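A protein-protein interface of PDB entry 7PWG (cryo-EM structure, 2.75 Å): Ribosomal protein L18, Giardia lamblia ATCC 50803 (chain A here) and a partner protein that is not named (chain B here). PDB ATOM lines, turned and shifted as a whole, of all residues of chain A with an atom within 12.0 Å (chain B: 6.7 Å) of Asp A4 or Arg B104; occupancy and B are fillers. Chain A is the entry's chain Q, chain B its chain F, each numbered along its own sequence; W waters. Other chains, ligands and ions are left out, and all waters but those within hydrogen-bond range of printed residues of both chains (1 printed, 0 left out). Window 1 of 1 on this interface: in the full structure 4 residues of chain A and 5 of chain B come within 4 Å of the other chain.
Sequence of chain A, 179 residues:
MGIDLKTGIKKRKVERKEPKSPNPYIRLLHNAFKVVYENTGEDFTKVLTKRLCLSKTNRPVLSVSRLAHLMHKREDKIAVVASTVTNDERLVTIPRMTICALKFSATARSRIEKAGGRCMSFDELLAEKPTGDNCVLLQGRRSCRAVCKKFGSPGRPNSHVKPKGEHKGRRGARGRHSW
Of the 14 printed residues of chain B, 5 touch a printed residue of chain A. Along chain B the printed residues that touch a printed residue of chain A span positions 87 to 105. Of the 10 printed residues of chain A, 4 touch a printed residue of chain B. Among the printed residues, 8 pairs touch across the chains. Among the printed residues, no Asp or Glu carboxylate lies within 4 Å of a Lys or Arg side-chain nitrogen of the other chain.
O of Gly A2 lies within hydrogen-bond range of NE2 of Gln B105, at 3.3 Å. The guanidinium group of Arg B104 lies close to the backbone carbonyl oxygen of Asp A4 (3.2 Å). O of Thr A7 lies within hydrogen-bond range of NH1 of Arg B104 (3.2 Å).
Of the printed residues of chain B, Asp A4 touches Arg B104 (3.2 Å). Of chain A, only Ile A3 (3.5 Å), Asp A4 (3.2 Å) and Thr A7 (3.2 Å) come within 4 Å of Arg B104. Leu B98 touches none of the printed residues of chain A. Gln B105 touches one residue of chain A. No residue of chain A comes within 4 Å of Asn B108. Of the printed residues of chain B, Thr A7 touches Arg B95 (3.6 Å), Ser B99 (3.8 Å) and Arg B104 (3.2 Å). Of the printed residues of chain B, Gly A2 touches Ile B87 and Gln B105. Printed residues of chain B within 4 Å of Ile A3: Ile B87 and Arg B104. Ile A9 touches none of the printed residues of chain B. Leu B101 touches none of the printed residues of chain A. The nearest printed residue of chain B that does not touch Thr A7 is Leu B98 (6.6 Å).
Water W1 lies within hydrogen-bond range of the backbone carbonyl oxygen of Arg B95 and the side-chain carboxylate of Asp A4.
C of Gly A2 touches CD1 of Ile B87, at 3.9 Å. N of Ile A3 touches CD1 of Ile B87, 3.8 Å away. Arg B104 touches Ile A3 (O to CD1, 3.5 Å). Arg B95 touches Thr A7. CB of Ser B99 touches CG2 of Thr A7, 3.8 Å away.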
ATOM      1  N   GLY A   2      -8.137  19.886   8.661  1.00  0.00           N
ATOM      2  CA  GLY A   2      -9.244  19.605   9.550  1.00  0.00           C
ATOM      3  C   GLY A   2     -10.048  18.373   9.196  1.00  0.00           C
ATOM      4  O   GLY A   2     -10.015  17.886   8.075  1.00  0.00           O
ATOM      5  N   ILE A   3     -10.785  17.868  10.175  1.00  0.00           N
ATOM      6  CA  ILE A   3     -11.607  16.674  10.029  1.00  0.00           C
ATOM      7  C   ILE A   3     -12.911  16.943  10.765  1.00  0.00           C
ATOM      8  O   ILE A   3     -12.896  17.510  11.859  1.00  0.00           O
ATOM      9  CB  ILE A   3     -10.858  15.430  10.570  1.00  0.00           C
ATOM     10  CG1 ILE A   3     -11.732  14.184  10.586  1.00  0.00           C
ATOM     11  CG2 ILE A   3     -10.302  15.693  11.960  1.00  0.00           C
ATOM     12  CD1 ILE A   3     -12.176  13.750   9.249  1.00  0.00           C
ATOM     13  N   ASP A   4     -14.040  16.574  10.169  1.00  0.00           N
ATOM     14  CA  ASP A   4     -15.350  16.803  10.800  1.00  0.00           C
ATOM     15  C   ASP A   4     -15.786  15.545  11.541  1.00  0.00           C
ATOM     16  O   ASP A   4     -16.306  14.608  10.941  1.00  0.00           O
ATOM     17  CB  ASP A   4     -16.411  17.216   9.787  1.00  0.00           C
ATOM     18  CG  ASP A   4     -17.814  17.258  10.397  1.00  0.00           C
ATOM     19  OD1 ASP A   4     -18.008  17.922  11.440  1.00  0.00           O
ATOM     20  OD2 ASP A   4     -18.728  16.612   9.854  1.00  0.00           O
ATOM     21  N   LEU A   5     -15.600  15.536  12.853  1.00  0.00           N
ATOM     22  CA  LEU A   5     -15.961  14.402  13.690  1.00  0.00           C
ATOM     23  C   LEU A   5     -17.036  14.775  14.700  1.00  0.00           C
ATOM     24  O   LEU A   5     -17.033  14.300  15.830  1.00  0.00           O
ATOM     25  CB  LEU A   5     -14.745  13.843  14.418  1.00  0.00           C
ATOM     26  CG  LEU A   5     -13.546  13.346  13.618  1.00  0.00           C
ATOM     27  CD1 LEU A   5     -12.402  13.087  14.555  1.00  0.00           C
ATOM     28  CD2 LEU A   5     -13.879  12.106  12.813  1.00  0.00           C
ATOM     29  N   LYS A   6     -17.971  15.630  14.306  1.00  0.00           N
ATOM     30  CA  LYS A   6     -19.064  16.042  15.177  1.00  0.00           C
ATOM     31  C   LYS A   6     -20.420  15.508  14.762  1.00  0.00           C
ATOM     32  O   LYS A   6     -21.195  15.104  15.622  1.00  0.00           O
ATOM     33  CB  LYS A   6     -19.133  17.565  15.251  1.00  0.00           C
ATOM     34  CG  LYS A   6     -17.840  18.186  15.706  1.00  0.00           C
ATOM     35  CD  LYS A   6     -17.960  19.680  15.928  1.00  0.00           C
ATOM     36  CE  LYS A   6     -16.634  20.275  16.334  1.00  0.00           C
ATOM     37  NZ  LYS A   6     -16.757  21.622  16.936  1.00  0.00           N
ATOM     38  N   THR A   7     -20.739  15.486  13.472  1.00  0.00           N
ATOM     39  CA  THR A   7     -22.087  15.139  13.047  1.00  0.00           C
ATOM     40  C   THR A   7     -22.264  13.628  13.029  1.00  0.00           C
ATOM     41  O   THR A   7     -21.401  12.889  12.550  1.00  0.00           O
ATOM     42  CB  THR A   7     -22.397  15.736  11.669  1.00  0.00           C
ATOM     43  OG1 THR A   7     -23.645  15.240  11.183  1.00  0.00           O
ATOM     44  CG2 THR A   7     -21.355  15.373  10.692  1.00  0.00           C
ATOM     45  N   GLY A   8     -23.393  13.175  13.563  1.00  0.00           N
ATOM     46  CA  GLY A   8     -23.652  11.759  13.674  1.00  0.00           C
ATOM     47  C   GLY A   8     -22.863  11.038  14.740  1.00  0.00           C
ATOM     48  O   GLY A   8     -22.858   9.811  14.742  1.00  0.00           O
ATOM     49  N   ILE A   9     -22.190  11.753  15.640  1.00  0.00           N
ATOM     50  CA  ILE A   9     -21.324  11.150  16.652  1.00  0.00           C
ATOM     51  C   ILE A   9     -21.617  11.794  17.998  1.00  0.00           C
ATOM     52  O   ILE A   9     -21.767  13.016  18.089  1.00  0.00           O
ATOM     53  CB  ILE A   9     -19.835  11.309  16.295  1.00  0.00           C
ATOM     54  CG1 ILE A   9     -19.476  10.442  15.091  1.00  0.00           C
ATOM     55  CG2 ILE A   9     -18.964  10.998  17.486  1.00  0.00           C
ATOM     56  CD1 ILE A   9     -18.058  10.592  14.643  1.00  0.00           C
ATOM     57  N   LYS A  10     -21.679  10.980  19.042  1.00  0.00           N
ATOM     58  CA  LYS A  10     -22.089  11.429  20.364  1.00  0.00           C
ATOM     59  C   LYS A  10     -20.911  11.449  21.326  1.00  0.00           C
ATOM     60  O   LYS A  10     -19.821  10.976  21.021  1.00  0.00           O
ATOM     61  CB  LYS A  10     -23.213  10.542  20.895  1.00  0.00           C
ATOM     62  CG  LYS A  10     -24.423  10.538  20.003  1.00  0.00           C
ATOM     63  CD  LYS A  10     -25.643  10.015  20.734  1.00  0.00           C
ATOM     64  CE  LYS A  10     -26.881  10.105  19.878  1.00  0.00           C
ATOM     65  NZ  LYS A  10     -27.004   8.952  18.972  1.00  0.00           N
ATOM     66  N   LYS A  11     -21.139  12.033  22.498  1.00  0.00           N
ATOM     67  CA  LYS A  11     -20.094  12.141  23.508  1.00  0.00           C
ATOM     68  C   LYS A  11     -19.908  10.810  24.232  1.00  0.00           C
ATOM     69  O   LYS A  11     -20.879  10.130  24.571  1.00  0.00           O
ATOM     70  CB  LYS A  11     -20.431  13.245  24.503  1.00  0.00           C
ATOM     71  CG  LYS A  11     -19.489  13.332  25.676  1.00  0.00           C
ATOM     72  CD  LYS A  11     -19.831  14.472  26.590  1.00  0.00           C
ATOM     73  CE  LYS A  11     -19.175  14.299  27.941  1.00  0.00           C
ATOM     74  NZ  LYS A  11     -19.182  15.540  28.750  1.00  0.00           N
ATOM     75  N   ARG B  83     -14.274  14.707  -2.353  1.00  0.00           N
ATOM     76  CA  ARG B  83     -14.590  15.962  -1.675  1.00  0.00           C
ATOM     77  C   ARG B  83     -13.525  16.989  -2.039  1.00  0.00           C
ATOM     78  O   ARG B  83     -12.356  16.644  -2.172  1.00  0.00           O
ATOM     79  CB  ARG B  83     -14.666  15.752  -0.157  1.00  0.00           C
ATOM     80  CG  ARG B  83     -15.006  17.001   0.643  1.00  0.00           C
ATOM     81  CD  ARG B  83     -15.526  16.761   2.063  1.00  0.00           C
ATOM     82  NE  ARG B  83     -15.824  18.050   2.684  1.00  0.00           N
ATOM     83  CZ  ARG B  83     -16.578  18.262   3.758  1.00  0.00           C
ATOM     84  NH1 ARG B  83     -16.752  19.493   4.187  1.00  0.00           N
ATOM     85  NH2 ARG B  83     -17.169  17.271   4.392  1.00  0.00           N
ATOM     86  N   ILE B  87     -14.152  22.303   5.803  1.00  0.00           N
ATOM     87  CA  ILE B  87     -15.148  22.129   6.861  1.00  0.00           C
ATOM     88  C   ILE B  87     -15.635  23.426   7.496  1.00  0.00           C
ATOM     89  O   ILE B  87     -16.545  23.368   8.331  1.00  0.00           O
ATOM     90  CB  ILE B  87     -14.636  21.181   7.968  1.00  0.00           C
ATOM     91  CG1 ILE B  87     -13.464  21.814   8.717  1.00  0.00           C
ATOM     92  CG2 ILE B  87     -14.264  19.835   7.392  1.00  0.00           C
ATOM     93  CD1 ILE B  87     -12.940  20.989   9.817  1.00  0.00           C
ATOM     94  N   ARG B  95     -24.002  19.167   5.626  1.00  0.00           N
ATOM     95  CA  ARG B  95     -23.020  18.392   6.378  1.00  0.00           C
ATOM     96  C   ARG B  95     -23.543  17.041   6.861  1.00  0.00           C
ATOM     97  O   ARG B  95     -22.736  16.155   7.108  1.00  0.00           O
ATOM     98  CB  ARG B  95     -22.465  19.205   7.553  1.00  0.00           C
ATOM     99  CG  ARG B  95     -23.431  19.626   8.607  1.00  0.00           C
ATOM    100  CD  ARG B  95     -22.673  20.278   9.748  1.00  0.00           C
ATOM    101  NE  ARG B  95     -23.545  20.891  10.741  1.00  0.00           N
ATOM    102  CZ  ARG B  95     -24.152  20.230  11.716  1.00  0.00           C
ATOM    103  NH1 ARG B  95     -24.928  20.874  12.572  1.00  0.00           N
ATOM    104  NH2 ARG B  95     -23.991  18.920  11.830  1.00  0.00           N
ATOM    105  N   LEU B  98     -23.072  14.734   3.638  1.00  0.00           N
ATOM    106  CA  LEU B  98     -21.668  14.394   3.455  1.00  0.00           C
ATOM    107  C   LEU B  98     -21.174  13.354   4.454  1.00  0.00           C
ATOM    108  O   LEU B  98     -20.232  12.620   4.153  1.00  0.00           O
ATOM    109  CB  LEU B  98     -20.821  15.653   3.556  1.00  0.00           C
ATOM    110  CG  LEU B  98     -20.794  16.599   2.363  1.00  0.00           C
ATOM    111  CD1 LEU B  98     -20.155  17.907   2.742  1.00  0.00           C
ATOM    112  CD2 LEU B  98     -20.074  15.945   1.197  1.00  0.00           C
ATOM    113  N   SER B  99     -21.755  13.290   5.649  1.00  0.00           N
ATOM    114  CA  SER B  99     -21.315  12.290   6.616  1.00  0.00           C
ATOM    115  C   SER B  99     -21.837  10.900   6.288  1.00  0.00           C
ATOM    116  O   SER B  99     -21.176   9.909   6.589  1.00  0.00           O
ATOM    117  CB  SER B  99     -21.738  12.697   8.022  1.00  0.00           C
ATOM    118  OG  SER B  99     -23.138  12.759   8.133  1.00  0.00           O
ATOM    119  N   LEU B 100     -23.024  10.804   5.699  1.00  0.00           N
ATOM    120  CA  LEU B 100     -23.542   9.514   5.272  1.00  0.00           C
ATOM    121  C   LEU B 100     -22.781   8.967   4.077  1.00  0.00           C
ATOM    122  O   LEU B 100     -22.726   7.752   3.889  1.00  0.00           O
ATOM    123  CB  LEU B 100     -25.022   9.631   4.948  1.00  0.00           C
ATOM    124  CG  LEU B 100     -25.933  10.111   6.073  1.00  0.00           C
ATOM    125  CD1 LEU B 100     -27.310  10.367   5.543  1.00  0.00           C
ATOM    126  CD2 LEU B 100     -25.971   9.114   7.207  1.00  0.00           C
ATOM    127  N   LEU B 101     -22.218   9.840   3.244  1.00  0.00           N
ATOM    128  CA  LEU B 101     -21.326   9.420   2.173  1.00  0.00           C
ATOM    129  C   LEU B 101     -19.937   9.113   2.677  1.00  0.00           C
ATOM    130  O   LEU B 101     -19.109   8.653   1.892  1.00  0.00           O
ATOM    131  CB  LEU B 101     -21.219  10.490   1.089  1.00  0.00           C
ATOM    132  CG  LEU B 101     -22.450  10.907   0.300  1.00  0.00           C
ATOM    133  CD1 LEU B 101     -22.172  12.189  -0.452  1.00  0.00           C
ATOM    134  CD2 LEU B 101     -22.848   9.824  -0.635  1.00  0.00           C
ATOM    135  N   ARG B 102     -19.669   9.373   3.951  1.00  0.00           N
ATOM    136  CA  ARG B 102     -18.373   9.135   4.570  1.00  0.00           C
ATOM    137  C   ARG B 102     -17.284  10.010   3.949  1.00  0.00           C
ATOM    138  O   ARG B 102     -16.189   9.550   3.653  1.00  0.00           O
ATOM    139  CB  ARG B 102     -17.995   7.655   4.495  1.00  0.00           C
ATOM    140  CG  ARG B 102     -19.016   6.697   5.087  1.00  0.00           C
ATOM    141  CD  ARG B 102     -18.430   5.303   5.189  1.00  0.00           C
ATOM    142  NE  ARG B 102     -18.163   4.712   3.889  1.00  0.00           N
ATOM    143  CZ  ARG B 102     -17.336   3.695   3.693  1.00  0.00           C
ATOM    144  NH1 ARG B 102     -16.682   3.167   4.712  1.00  0.00           N
ATOM    145  NH2 ARG B 102     -17.142   3.211   2.477  1.00  0.00           N
ATOM    146  N   LEU B 103     -17.593  11.290   3.769  1.00  0.00           N
ATOM    147  CA  LEU B 103     -16.675  12.278   3.207  1.00  0.00           C
ATOM    148  C   LEU B 103     -16.498  13.379   4.244  1.00  0.00           C
ATOM    149  O   LEU B 103     -17.193  14.395   4.220  1.00  0.00           O
ATOM    150  CB  LEU B 103     -17.188  12.815   1.896  1.00  0.00           C
ATOM    151  CG  LEU B 103     -17.134  11.872   0.697  1.00  0.00           C
ATOM    152  CD1 LEU B 103     -17.640  12.571  -0.538  1.00  0.00           C
ATOM    153  CD2 LEU B 103     -15.729  11.308   0.455  1.00  0.00           C
ATOM    154  N   ARG B 104     -15.556  13.175   5.153  1.00  0.00           N
ATOM    155  CA  ARG B 104     -15.357  14.061   6.282  1.00  0.00           C
ATOM    156  C   ARG B 104     -14.110  14.921   6.171  1.00  0.00           C
ATOM    157  O   ARG B 104     -13.936  15.824   6.986  1.00  0.00           O
ATOM    158  CB  ARG B 104     -15.298  13.250   7.587  1.00  0.00           C
ATOM    159  CG  ARG B 104     -16.574  12.516   7.947  1.00  0.00           C
ATOM    160  CD  ARG B 104     -16.483  11.882   9.319  1.00  0.00           C
ATOM    161  NE  ARG B 104     -17.597  10.990   9.616  1.00  0.00           N
ATOM    162  CZ  ARG B 104     -18.623  11.301  10.404  1.00  0.00           C
ATOM    163  NH1 ARG B 104     -18.686  12.485  10.983  1.00  0.00           N
ATOM    164  NH2 ARG B 104     -19.588  10.425  10.612  1.00  0.00           N
ATOM    165  N   GLN B 105     -13.250  14.679   5.191  1.00  0.00           N
ATOM    166  CA  GLN B 105     -12.017  15.429   5.034  1.00  0.00           C
ATOM    167  C   GLN B 105     -11.861  15.834   3.575  1.00  0.00           C
ATOM    168  O   GLN B 105     -12.378  15.178   2.677  1.00  0.00           O
ATOM    169  CB  GLN B 105     -10.828  14.618   5.523  1.00  0.00           C
ATOM    170  CG  GLN B 105      -9.548  15.378   5.603  1.00  0.00           C
ATOM    171  CD  GLN B 105      -8.518  14.691   6.443  1.00  0.00           C
ATOM    172  OE1 GLN B 105      -8.226  13.516   6.257  1.00  0.00           O
ATOM    173  NE2 GLN B 105      -7.956  15.424   7.383  1.00  0.00           N
ATOM    174  N   ILE B 106     -11.108  16.917   3.351  1.00  0.00           N
ATOM    175  CA  ILE B 106     -11.181  17.665   2.103  1.00  0.00           C
ATOM    176  C   ILE B 106     -10.688  16.898   0.879  1.00  0.00           C
ATOM    177  O   ILE B 106     -11.110  17.220  -0.226  1.00  0.00           O
ATOM    178  CB  ILE B 106     -10.437  19.012   2.217  1.00  0.00           C
ATOM    179  CG1 ILE B 106     -10.593  19.817   0.927  1.00  0.00           C
ATOM    180  CG2 ILE B 106      -8.971  18.830   2.596  1.00  0.00           C
ATOM    181  CD1 ILE B 106      -9.409  20.646   0.561  1.00  0.00           C
ATOM    182  N   ASN B 108     -10.764  13.311   0.544  1.00  0.00           N
ATOM    183  CA  ASN B 108     -11.146  11.909   0.645  1.00  0.00           C
ATOM    184  C   ASN B 108     -12.034  11.493  -0.526  1.00  0.00           C
ATOM    185  O   ASN B 108     -12.725  12.307  -1.136  1.00  0.00           O
ATOM    186  CB  ASN B 108     -11.870  11.652   1.966  1.00  0.00           C
ATOM    187  CG  ASN B 108     -10.981  11.864   3.179  1.00  0.00           C
ATOM    188  OD1 ASN B 108      -9.851  12.319   3.075  1.00  0.00           O
ATOM    189  ND2 ASN B 108     -11.499  11.522   4.339  1.00  0.00           N
ATOM    190  N   PRO B 199     -12.525   4.983   3.811  1.00  0.00           N
ATOM    191  CA  PRO B 199     -12.461   6.013   2.764  1.00  0.00           C
ATOM    192  C   PRO B 199     -11.027   6.362   2.377  1.00  0.00           C
ATOM    193  O   PRO B 199     -10.151   6.516   3.226  1.00  0.00           O
ATOM    194  CB  PRO B 199     -13.175   7.201   3.407  1.00  0.00           C
ATOM    195  CG  PRO B 199     -14.111   6.572   4.362  1.00  0.00           C
ATOM    196  CD  PRO B 199     -13.410   5.384   4.911  1.00  0.00           C
HETATM  197  O   HOH W   1     -19.869  16.702   6.948  1.00  0.00           O
